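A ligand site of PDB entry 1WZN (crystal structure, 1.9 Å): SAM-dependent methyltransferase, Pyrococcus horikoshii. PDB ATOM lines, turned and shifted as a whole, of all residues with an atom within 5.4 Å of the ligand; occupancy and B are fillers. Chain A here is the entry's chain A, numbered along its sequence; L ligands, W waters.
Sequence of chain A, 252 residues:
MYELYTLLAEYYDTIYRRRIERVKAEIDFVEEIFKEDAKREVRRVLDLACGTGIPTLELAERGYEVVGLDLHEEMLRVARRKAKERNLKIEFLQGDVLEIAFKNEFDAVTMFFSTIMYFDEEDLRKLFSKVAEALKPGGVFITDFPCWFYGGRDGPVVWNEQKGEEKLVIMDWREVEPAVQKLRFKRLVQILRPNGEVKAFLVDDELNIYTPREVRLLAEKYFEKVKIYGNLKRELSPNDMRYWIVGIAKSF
A sulfur (S1) of the ligand lies close to the side-chain hydroxyl (OH) of Tyr 12, 3.3 Å away. An oxygen (O4) of the ligand is in hydrogen-bond range of the side-chain carboxylate (OD2) of Asp 70 (2.6 Å). OD1 of Asp 96 sits at hydrogen-bond distance from N4 of the ligand (2.9 Å). N of Leu 71 lies within hydrogen-bond range of N6 of the ligand (3.2 Å). The backbone carbonyl oxygen (O) of Phe 112 sits at hydrogen-bond distance from a nitrogen (N1) of the ligand. OH of Tyr 5 lies close to S1 of the ligand, 3.7 Å away. A nitrogen (N5) of the ligand is in hydrogen-bond range of the backbone NH (N) of Val 97. The backbone carbonyl oxygen (O) of Ala 49 is in hydrogen-bond range of a nitrogen (N1) of the ligand (2.9 Å). An oxygen (O1) of the ligand lies within salt-bridge range of the guanidinium group (NH2) of Arg 19, at 2.9 Å. O5 of the ligand lies within hydrogen-bond range of ND1 of His 72, at 2.8 Å.
N of Leu 98 is in hydrogen-bond range of OD1 of Asp 96 (2.9 Å). The backbone NH of Gly 51 lies within hydrogen-bond range of the side-chain carboxylate of Asp 70, 2.8 Å away. The side-chain carboxylate (OD1) of Asp 70 sits at hydrogen-bond distance from the backbone NH (N) of His 72. The backbone NH (N) of Cys 50 is in hydrogen-bond range of the side-chain carboxylate (OD2) of Asp 70. The backbone NH (N) of Ala 49 sits at hydrogen-bond distance from the backbone carbonyl oxygen (O) of Leu 69 (2.7 Å). The backbone NH of Leu 71 is in hydrogen-bond range of the backbone carbonyl oxygen of Gly 95, at 3.3 Å. OH of Tyr 5 lies within hydrogen-bond range of OH of Tyr 118, at 2.7 Å. N of Cys 50 sits at hydrogen-bond distance from O of Leu 69.
Cys 50 touches the ligand (O to C1, 3.4 Å). CA of Gly 51 touches O4 of the ligand, at 3.2 Å. CD1 of Ile 54 touches O2 of the ligand, at 3.9 Å. Pro 55 touches the ligand. Met 75 touches the ligand. Gly 95 touches the ligand (O to C13, 3.4 Å). Phe 113 touches the ligand. Thr 115 touches the ligand (OG1 to C5, 3.5 Å). Phe 119 touches the ligand (CE1 to N4, 3.6 Å). Of the 27 residues printed, 19 come within 4 Å of the ligand. The nearest printed residue that does not touch the ligand is Tyr 2 (4.3 Å).
Water W6 bridges OH of Tyr 2 (2.6 Å) and N3 of the ligand (2.7 Å). Water W4 lies within hydrogen-bond range of N1 of the ligand (2.7 Å), OD2 of Asp 47 (2.8 Å) and O of Cys 50 (2.9 Å). Water W3 lies within hydrogen-bond range of OG1 of Thr 52 (2.7 Å), O2 of the ligand (2.8 Å), N of Ile 54 (3.1 Å) and N of Gly 53 (3.2 Å).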
ATOM      1  N   TYR A   2       2.467 -11.896  11.269  1.00  0.00           N
ATOM      2  CA  TYR A   2       1.038 -11.657  11.464  1.00  0.00           C
ATOM      3  C   TYR A   2       0.652 -11.090  12.831  1.00  0.00           C
ATOM      4  O   TYR A   2      -0.529 -11.036  13.157  1.00  0.00           O
ATOM      5  CB  TYR A   2       0.237 -12.935  11.217  1.00  0.00           C
ATOM      6  CG  TYR A   2       0.493 -13.604   9.889  1.00  0.00           C
ATOM      7  CD1 TYR A   2       0.535 -12.870   8.701  1.00  0.00           C
ATOM      8  CD2 TYR A   2       0.658 -14.991   9.813  1.00  0.00           C
ATOM      9  CE1 TYR A   2       0.720 -13.493   7.472  1.00  0.00           C
ATOM     10  CE2 TYR A   2       0.851 -15.625   8.587  1.00  0.00           C
ATOM     11  CZ  TYR A   2       0.878 -14.870   7.415  1.00  0.00           C
ATOM     12  OH  TYR A   2       1.038 -15.510   6.207  1.00  0.00           O
ATOM     13  N   TYR A   5      -2.145  -8.695  12.841  1.00  0.00           N
ATOM     14  CA  TYR A   5      -3.489  -9.191  12.535  1.00  0.00           C
ATOM     15  C   TYR A   5      -4.100 -10.120  13.579  1.00  0.00           C
ATOM     16  O   TYR A   5      -5.229 -10.583  13.429  1.00  0.00           O
ATOM     17  CB  TYR A   5      -3.450  -9.881  11.182  1.00  0.00           C
ATOM     18  CG  TYR A   5      -2.699  -9.061  10.174  1.00  0.00           C
ATOM     19  CD1 TYR A   5      -3.000  -7.714   9.999  1.00  0.00           C
ATOM     20  CD2 TYR A   5      -1.662  -9.610   9.413  1.00  0.00           C
ATOM     21  CE1 TYR A   5      -2.296  -6.924   9.102  1.00  0.00           C
ATOM     22  CE2 TYR A   5      -0.955  -8.830   8.506  1.00  0.00           C
ATOM     23  CZ  TYR A   5      -1.273  -7.482   8.366  1.00  0.00           C
ATOM     24  OH  TYR A   5      -0.571  -6.683   7.501  1.00  0.00           O
ATOM     25  N   TYR A  12      -5.679  -2.251  14.958  1.00  0.00           N
ATOM     26  CA  TYR A  12      -5.434  -2.006  13.533  1.00  0.00           C
ATOM     27  C   TYR A  12      -6.066  -0.710  13.013  1.00  0.00           C
ATOM     28  O   TYR A  12      -5.410   0.084  12.337  1.00  0.00           O
ATOM     29  CB  TYR A  12      -5.949  -3.193  12.700  1.00  0.00           C
ATOM     30  CG  TYR A  12      -5.523  -3.130  11.241  1.00  0.00           C
ATOM     31  CD1 TYR A  12      -4.269  -3.609  10.835  1.00  0.00           C
ATOM     32  CD2 TYR A  12      -6.358  -2.563  10.284  1.00  0.00           C
ATOM     33  CE1 TYR A  12      -3.876  -3.518   9.504  1.00  0.00           C
ATOM     34  CE2 TYR A  12      -5.963  -2.462   8.954  1.00  0.00           C
ATOM     35  CZ  TYR A  12      -4.717  -2.941   8.566  1.00  0.00           C
ATOM     36  OH  TYR A  12      -4.319  -2.822   7.259  1.00  0.00           O
ATOM     37  N   ARG A  19      -5.485   5.768   6.809  1.00  0.00           N
ATOM     38  CA  ARG A  19      -6.015   4.957   5.720  1.00  0.00           C
ATOM     39  C   ARG A  19      -7.532   5.014   5.666  1.00  0.00           C
ATOM     40  O   ARG A  19      -8.154   4.970   4.610  1.00  0.00           O
ATOM     41  CB  ARG A  19      -5.547   3.517   5.932  1.00  0.00           C
ATOM     42  CG  ARG A  19      -5.741   2.647   4.682  1.00  0.00           C
ATOM     43  CD  ARG A  19      -6.818   1.572   4.888  1.00  0.00           C
ATOM     44  NE  ARG A  19      -6.794   0.602   3.798  1.00  0.00           N
ATOM     45  CZ  ARG A  19      -7.483   0.910   2.682  1.00  0.00           C
ATOM     46  NH1 ARG A  19      -8.145   2.049   2.605  1.00  0.00           N
ATOM     47  NH2 ARG A  19      -7.501   0.055   1.659  1.00  0.00           N
ATOM     48  N   ASP A  47     -13.695  -9.424  -1.730  1.00  0.00           N
ATOM     49  CA  ASP A  47     -12.572  -8.639  -1.213  1.00  0.00           C
ATOM     50  C   ASP A  47     -11.635  -9.578  -0.444  1.00  0.00           C
ATOM     51  O   ASP A  47     -11.924  -9.978   0.676  1.00  0.00           O
ATOM     52  CB  ASP A  47     -13.082  -7.510  -0.311  1.00  0.00           C
ATOM     53  CG  ASP A  47     -11.972  -6.575   0.132  1.00  0.00           C
ATOM     54  OD1 ASP A  47     -11.016  -6.386  -0.658  1.00  0.00           O
ATOM     55  OD2 ASP A  47     -12.048  -6.037   1.260  1.00  0.00           O
ATOM     56  N   LEU A  48     -10.514  -9.926  -1.081  1.00  0.00           N
ATOM     57  CA  LEU A  48      -9.522 -10.841  -0.509  1.00  0.00           C
ATOM     58  C   LEU A  48      -8.600 -10.186   0.513  1.00  0.00           C
ATOM     59  O   LEU A  48      -8.133  -9.064   0.306  1.00  0.00           O
ATOM     60  CB  LEU A  48      -8.686 -11.441  -1.653  1.00  0.00           C
ATOM     61  CG  LEU A  48      -9.469 -12.197  -2.751  1.00  0.00           C
ATOM     62  CD1 LEU A  48      -8.532 -12.528  -3.918  1.00  0.00           C
ATOM     63  CD2 LEU A  48     -10.060 -13.483  -2.191  1.00  0.00           C
ATOM     64  N   ALA A  49      -8.306 -10.910   1.593  1.00  0.00           N
ATOM     65  CA  ALA A  49      -7.467 -10.410   2.700  1.00  0.00           C
ATOM     66  C   ALA A  49      -8.088  -9.088   3.137  1.00  0.00           C
ATOM     67  O   ALA A  49      -7.412  -8.062   3.207  1.00  0.00           O
ATOM     68  CB  ALA A  49      -6.017 -10.227   2.243  1.00  0.00           C
ATOM     69  N   CYS A  50      -9.384  -9.145   3.444  1.00  0.00           N
ATOM     70  CA  CYS A  50     -10.162  -7.964   3.820  1.00  0.00           C
ATOM     71  C   CYS A  50      -9.842  -7.295   5.144  1.00  0.00           C
ATOM     72  O   CYS A  50     -10.313  -6.180   5.389  1.00  0.00           O
ATOM     73  CB  CYS A  50     -11.655  -8.289   3.784  1.00  0.00           C
ATOM     74  SG  CYS A  50     -12.153  -9.514   5.006  1.00  0.00           S
ATOM     75  N   GLY A  51      -9.086  -7.964   6.010  1.00  0.00           N
ATOM     76  CA  GLY A  51      -8.745  -7.377   7.301  1.00  0.00           C
ATOM     77  C   GLY A  51      -9.969  -6.940   8.098  1.00  0.00           C
ATOM     78  O   GLY A  51     -10.940  -7.680   8.182  1.00  0.00           O
ATOM     79  N   THR A  52      -9.898  -5.740   8.686  1.00  0.00           N
ATOM     80  CA  THR A  52     -11.003  -5.191   9.472  1.00  0.00           C
ATOM     81  C   THR A  52     -12.112  -4.640   8.562  1.00  0.00           C
ATOM     82  O   THR A  52     -13.062  -4.015   9.032  1.00  0.00           O
ATOM     83  CB  THR A  52     -10.534  -4.052  10.382  1.00  0.00           C
ATOM     84  OG1 THR A  52     -10.062  -2.963   9.581  1.00  0.00           O
ATOM     85  CG2 THR A  52      -9.428  -4.544  11.322  1.00  0.00           C
ATOM     86  N   GLY A  53     -11.956  -4.875   7.257  1.00  0.00           N
ATOM     87  CA  GLY A  53     -12.966  -4.450   6.297  1.00  0.00           C
ATOM     88  C   GLY A  53     -13.122  -2.978   5.989  1.00  0.00           C
ATOM     89  O   GLY A  53     -14.209  -2.537   5.601  1.00  0.00           O
ATOM     90  N   ILE A  54     -12.042  -2.201   6.143  1.00  0.00           N
ATOM     91  CA  ILE A  54     -12.086  -0.771   5.867  1.00  0.00           C
ATOM     92  C   ILE A  54     -12.690  -0.481   4.492  1.00  0.00           C
ATOM     93  O   ILE A  54     -13.721   0.185   4.392  1.00  0.00           O
ATOM     94  CB  ILE A  54     -10.674  -0.146   6.037  1.00  0.00           C
ATOM     95  CG1 ILE A  54     -10.310  -0.136   7.525  1.00  0.00           C
ATOM     96  CG2 ILE A  54     -10.646   1.270   5.484  1.00  0.00           C
ATOM     97  CD1 ILE A  54      -8.867   0.200   7.836  1.00  0.00           C
ATOM     98  N   PRO A  55     -12.069  -0.966   3.400  1.00  0.00           N
ATOM     99  CA  PRO A  55     -12.696  -0.667   2.103  1.00  0.00           C
ATOM    100  C   PRO A  55     -13.929  -1.552   1.845  1.00  0.00           C
ATOM    101  O   PRO A  55     -14.812  -1.182   1.068  1.00  0.00           O
ATOM    102  CB  PRO A  55     -11.562  -0.912   1.106  1.00  0.00           C
ATOM    103  CG  PRO A  55     -10.763  -2.003   1.767  1.00  0.00           C
ATOM    104  CD  PRO A  55     -10.730  -1.566   3.213  1.00  0.00           C
ATOM    105  N   LEU A  69     -12.878 -12.059   2.671  1.00  0.00           N
ATOM    106  CA  LEU A  69     -12.155 -13.245   3.120  1.00  0.00           C
ATOM    107  C   LEU A  69     -10.839 -12.860   3.791  1.00  0.00           C
ATOM    108  O   LEU A  69     -10.096 -12.030   3.277  1.00  0.00           O
ATOM    109  CB  LEU A  69     -11.848 -14.166   1.931  1.00  0.00           C
ATOM    110  CG  LEU A  69     -10.967 -15.377   2.202  1.00  0.00           C
ATOM    111  CD1 LEU A  69     -11.768 -16.464   2.914  1.00  0.00           C
ATOM    112  CD2 LEU A  69     -10.428 -15.913   0.884  1.00  0.00           C
ATOM    113  N   ASP A  70     -10.565 -13.443   4.948  1.00  0.00           N
ATOM    114  CA  ASP A  70      -9.306 -13.150   5.627  1.00  0.00           C
ATOM    115  C   ASP A  70      -8.814 -14.376   6.377  1.00  0.00           C
ATOM    116  O   ASP A  70      -9.602 -15.196   6.870  1.00  0.00           O
ATOM    117  CB  ASP A  70      -9.433 -11.939   6.564  1.00  0.00           C
ATOM    118  CG  ASP A  70      -8.071 -11.315   6.888  1.00  0.00           C
ATOM    119  OD1 ASP A  70      -7.393 -11.811   7.803  1.00  0.00           O
ATOM    120  OD2 ASP A  70      -7.683 -10.341   6.214  1.00  0.00           O
ATOM    121  N   LEU A  71      -7.500 -14.510   6.447  1.00  0.00           N
ATOM    122  CA  LEU A  71      -6.872 -15.623   7.128  1.00  0.00           C
ATOM    123  C   LEU A  71      -7.071 -15.566   8.636  1.00  0.00           C
ATOM    124  O   LEU A  71      -7.183 -16.598   9.297  1.00  0.00           O
ATOM    125  CB  LEU A  71      -5.365 -15.634   6.822  1.00  0.00           C
ATOM    126  CG  LEU A  71      -4.523 -16.777   7.394  1.00  0.00           C
ATOM    127  CD1 LEU A  71      -5.021 -18.117   6.838  1.00  0.00           C
ATOM    128  CD2 LEU A  71      -3.058 -16.572   7.010  1.00  0.00           C
ATOM    129  N   HIS A  72      -7.150 -14.358   9.188  1.00  0.00           N
ATOM    130  CA  HIS A  72      -7.276 -14.208  10.630  1.00  0.00           C
ATOM    131  C   HIS A  72      -8.634 -13.801  11.176  1.00  0.00           C
ATOM    132  O   HIS A  72      -9.164 -12.731  10.863  1.00  0.00           O
ATOM    133  CB  HIS A  72      -6.202 -13.229  11.121  1.00  0.00           C
ATOM    134  CG  HIS A  72      -4.811 -13.701  10.857  1.00  0.00           C
ATOM    135  ND1 HIS A  72      -4.068 -13.261   9.774  1.00  0.00           N
ATOM    136  CD2 HIS A  72      -4.040 -14.611  11.491  1.00  0.00           C
ATOM    137  CE1 HIS A  72      -2.901 -13.883   9.772  1.00  0.00           C
ATOM    138  NE2 HIS A  72      -2.863 -14.711  10.799  1.00  0.00           N
ATOM    139  N   MET A  75      -9.119 -10.408  12.848  1.00  0.00           N
ATOM    140  CA  MET A  75      -9.400  -9.254  12.000  1.00  0.00           C
ATOM    141  C   MET A  75     -10.881  -9.252  11.610  1.00  0.00           C
ATOM    142  O   MET A  75     -11.542  -8.203  11.656  1.00  0.00           O
ATOM    143  CB  MET A  75      -8.535  -9.282  10.739  1.00  0.00           C
ATOM    144  CG  MET A  75      -7.040  -9.135  11.000  1.00  0.00           C
ATOM    145  SD  MET A  75      -6.592  -7.494  11.605  1.00  0.00           S
ATOM    146  CE  MET A  75      -6.642  -6.561  10.106  1.00  0.00           C
ATOM    147  N   GLY A  95     -10.256 -17.849   5.809  1.00  0.00           N
ATOM    148  CA  GLY A  95      -9.608 -18.756   4.880  1.00  0.00           C
ATOM    149  C   GLY A  95      -8.392 -18.113   4.238  1.00  0.00           C
ATOM    150  O   GLY A  95      -8.188 -16.904   4.337  1.00  0.00           O
ATOM    151  N   ASP A  96      -7.605 -18.940   3.573  1.00  0.00           N
ATOM    152  CA  ASP A  96      -6.390 -18.508   2.890  1.00  0.00           C
ATOM    153  C   ASP A  96      -6.789 -18.129   1.456  1.00  0.00           C
ATOM    154  O   ASP A  96      -7.495 -18.896   0.781  1.00  0.00           O
ATOM    155  CB  ASP A  96      -5.411 -19.686   2.852  1.00  0.00           C
ATOM    156  CG  ASP A  96      -4.026 -19.297   2.361  1.00  0.00           C
ATOM    157  OD1 ASP A  96      -3.902 -18.358   1.541  1.00  0.00           O
ATOM    158  OD2 ASP A  96      -3.055 -19.963   2.776  1.00  0.00           O
ATOM    159  N   VAL A  97      -6.371 -16.961   0.993  1.00  0.00           N
ATOM    160  CA  VAL A  97      -6.695 -16.528  -0.362  1.00  0.00           C
ATOM    161  C   VAL A  97      -6.136 -17.483  -1.409  1.00  0.00           C
ATOM    162  O   VAL A  97      -6.692 -17.586  -2.511  1.00  0.00           O
ATOM    163  CB  VAL A  97      -6.146 -15.098  -0.679  1.00  0.00           C
ATOM    164  CG1 VAL A  97      -6.800 -14.066   0.222  1.00  0.00           C
ATOM    165  CG2 VAL A  97      -4.638 -15.067  -0.543  1.00  0.00           C
ATOM    166  N   LEU A  98      -5.051 -18.184  -1.084  1.00  0.00           N
ATOM    167  CA  LEU A  98      -4.454 -19.121  -2.037  1.00  0.00           C
ATOM    168  C   LEU A  98      -5.263 -20.404  -2.176  1.00  0.00           C
ATOM    169  O   LEU A  98      -4.956 -21.247  -3.024  1.00  0.00           O
ATOM    170  CB  LEU A  98      -3.026 -19.462  -1.611  1.00  0.00           C
ATOM    171  CG  LEU A  98      -2.063 -18.274  -1.529  1.00  0.00           C
ATOM    172  CD1 LEU A  98      -0.693 -18.769  -1.073  1.00  0.00           C
ATOM    173  CD2 LEU A  98      -1.953 -17.592  -2.882  1.00  0.00           C
ATOM    174  N   PHE A 112      -6.940  -5.028  -1.266  1.00  0.00           N
ATOM    175  CA  PHE A 112      -6.509  -3.684  -0.896  1.00  0.00           C
ATOM    176  C   PHE A 112      -5.383  -3.552   0.109  1.00  0.00           C
ATOM    177  O   PHE A 112      -5.234  -4.372   1.023  1.00  0.00           O
ATOM    178  CB  PHE A 112      -7.707  -2.898  -0.358  1.00  0.00           C
ATOM    179  CG  PHE A 112      -8.792  -2.639  -1.373  1.00  0.00           C
ATOM    180  CD1 PHE A 112      -8.580  -1.732  -2.416  1.00  0.00           C
ATOM    181  CD2 PHE A 112     -10.019  -3.284  -1.278  1.00  0.00           C
ATOM    182  CE1 PHE A 112      -9.593  -1.481  -3.352  1.00  0.00           C
ATOM    183  CE2 PHE A 112     -11.027  -3.035  -2.201  1.00  0.00           C
ATOM    184  CZ  PHE A 112     -10.815  -2.127  -3.244  1.00  0.00           C
ATOM    185  N   PHE A 113      -4.605  -2.495  -0.094  1.00  0.00           N
ATOM    186  CA  PHE A 113      -3.509  -2.127   0.794  1.00  0.00           C
ATOM    187  C   PHE A 113      -2.237  -2.964   0.834  1.00  0.00           C
ATOM    188  O   PHE A 113      -1.854  -3.508   1.876  1.00  0.00           O
ATOM    189  CB  PHE A 113      -4.061  -1.920   2.211  1.00  0.00           C
ATOM    190  CG  PHE A 113      -3.196  -1.053   3.092  1.00  0.00           C
ATOM    191  CD1 PHE A 113      -2.592   0.096   2.585  1.00  0.00           C
ATOM    192  CD2 PHE A 113      -2.984  -1.372   4.426  1.00  0.00           C
ATOM    193  CE1 PHE A 113      -1.795   0.918   3.401  1.00  0.00           C
ATOM    194  CE2 PHE A 113      -2.186  -0.571   5.254  1.00  0.00           C
ATOM    195  CZ  PHE A 113      -1.596   0.581   4.729  1.00  0.00           C
ATOM    196  N   THR A 115      -1.301  -5.914   0.020  1.00  0.00           N
ATOM    197  CA  THR A 115      -1.225  -7.306   0.411  1.00  0.00           C
ATOM    198  C   THR A 115      -0.529  -8.271  -0.550  1.00  0.00           C
ATOM    199  O   THR A 115      -0.105  -9.340  -0.132  1.00  0.00           O
ATOM    200  CB  THR A 115      -2.626  -7.847   0.775  1.00  0.00           C
ATOM    201  OG1 THR A 115      -3.145  -7.054   1.856  1.00  0.00           O
ATOM    202  CG2 THR A 115      -2.555  -9.305   1.243  1.00  0.00           C
ATOM    203  N   TYR A 118       2.801  -9.968   0.543  1.00  0.00           N
ATOM    204  CA  TYR A 118       2.953 -11.112   1.430  1.00  0.00           C
ATOM    205  C   TYR A 118       3.241 -12.383   0.648  1.00  0.00           C
ATOM    206  O   TYR A 118       3.619 -13.404   1.230  1.00  0.00           O
ATOM    207  CB  TYR A 118       1.677 -11.320   2.269  1.00  0.00           C
ATOM    208  CG  TYR A 118       1.621 -10.477   3.511  1.00  0.00           C
ATOM    209  CD1 TYR A 118       2.291 -10.876   4.675  1.00  0.00           C
ATOM    210  CD2 TYR A 118       0.982  -9.246   3.521  1.00  0.00           C
ATOM    211  CE1 TYR A 118       2.318 -10.061   5.803  1.00  0.00           C
ATOM    212  CE2 TYR A 118       1.006  -8.419   4.636  1.00  0.00           C
ATOM    213  CZ  TYR A 118       1.677  -8.836   5.767  1.00  0.00           C
ATOM    214  OH  TYR A 118       1.733  -8.003   6.864  1.00  0.00           O
ATOM    215  N   PHE A 119       3.106 -12.332  -0.678  1.00  0.00           N
ATOM    216  CA  PHE A 119       3.313 -13.513  -1.512  1.00  0.00           C
ATOM    217  C   PHE A 119       4.524 -13.462  -2.423  1.00  0.00           C
ATOM    218  O   PHE A 119       4.783 -12.447  -3.070  1.00  0.00           O
ATOM    219  CB  PHE A 119       2.056 -13.713  -2.368  1.00  0.00           C
ATOM    220  CG  PHE A 119       0.786 -13.725  -1.575  1.00  0.00           C
ATOM    221  CD1 PHE A 119       0.457 -14.819  -0.794  1.00  0.00           C
ATOM    222  CD2 PHE A 119      -0.050 -12.613  -1.557  1.00  0.00           C
ATOM    223  CE1 PHE A 119      -0.696 -14.811   0.000  1.00  0.00           C
ATOM    224  CE2 PHE A 119      -1.198 -12.595  -0.772  1.00  0.00           C
ATOM    225  CZ  PHE A 119      -1.524 -13.698  -0.001  1.00  0.00           C
HETATM  226  N1  LIG L   1      -7.584  -5.155   2.945  1.00  0.00           N
HETATM  227  C1  LIG L   1      -7.474  -4.586   4.359  1.00  0.00           C
HETATM  228  C2  LIG L   1      -6.362  -5.134   5.215  1.00  0.00           C
HETATM  229  C3  LIG L   1      -4.908  -4.967   4.815  1.00  0.00           C
HETATM  230  S1  LIG L   1      -3.927  -5.867   6.101  1.00  0.00           S
HETATM  231  C4  LIG L   1      -7.367  -3.008   4.207  1.00  0.00           C
HETATM  232  O1  LIG L   1      -7.380  -2.492   3.064  1.00  0.00           O
HETATM  233  O2  LIG L   1      -7.287  -2.332   5.306  1.00  0.00           O
HETATM  234  C5  LIG L   1      -3.396  -7.331   5.292  1.00  0.00           C
HETATM  235  C6  LIG L   1      -4.434  -8.527   5.530  1.00  0.00           C
HETATM  236  O3  LIG L   1      -3.820  -9.617   4.831  1.00  0.00           O
HETATM  237  C7  LIG L   1      -4.582  -9.023   6.950  1.00  0.00           C
HETATM  238  O4  LIG L   1      -5.923  -8.868   7.398  1.00  0.00           O
HETATM  239  C8  LIG L   1      -4.073 -10.522   6.861  1.00  0.00           C
HETATM  240  O5  LIG L   1      -4.737 -11.372   7.789  1.00  0.00           O
HETATM  241  C9  LIG L   1      -4.339 -10.856   5.403  1.00  0.00           C
HETATM  242  N2  LIG L   1      -3.667 -11.895   4.864  1.00  0.00           N
HETATM  243  C10 LIG L   1      -2.309 -12.154   4.713  1.00  0.00           C
HETATM  244  N3  LIG L   1      -2.029 -13.274   4.134  1.00  0.00           N
HETATM  245  C11 LIG L   1      -3.301 -13.856   3.853  1.00  0.00           C
HETATM  246  C12 LIG L   1      -3.661 -15.093   3.216  1.00  0.00           C
HETATM  247  N4  LIG L   1      -2.764 -15.973   2.747  1.00  0.00           N
HETATM  248  N5  LIG L   1      -5.014 -15.317   3.122  1.00  0.00           N
HETATM  249  C13 LIG L   1      -5.959 -14.449   3.591  1.00  0.00           C
HETATM  250  N6  LIG L   1      -5.652 -13.251   4.203  1.00  0.00           N
HETATM  251  C14 LIG L   1      -4.311 -13.026   4.302  1.00  0.00           C
HETATM  252  O   HOH W   1      -5.608  -7.083   1.312  1.00  0.00           O
HETATM  253  O   HOH W   2       0.272 -16.709   2.557  1.00  0.00           O
HETATM  254  O   HOH W   3      -9.285  -3.193   7.020  1.00  0.00           O
HETATM  255  O   HOH W   4     -10.277  -4.709   2.926  1.00  0.00           O
HETATM  256  O   HOH W   5      -8.582  -6.368   0.580  1.00  0.00           O
HETATM  257  O   HOH W   6       0.306 -14.667   3.900  1.00  0.00           O
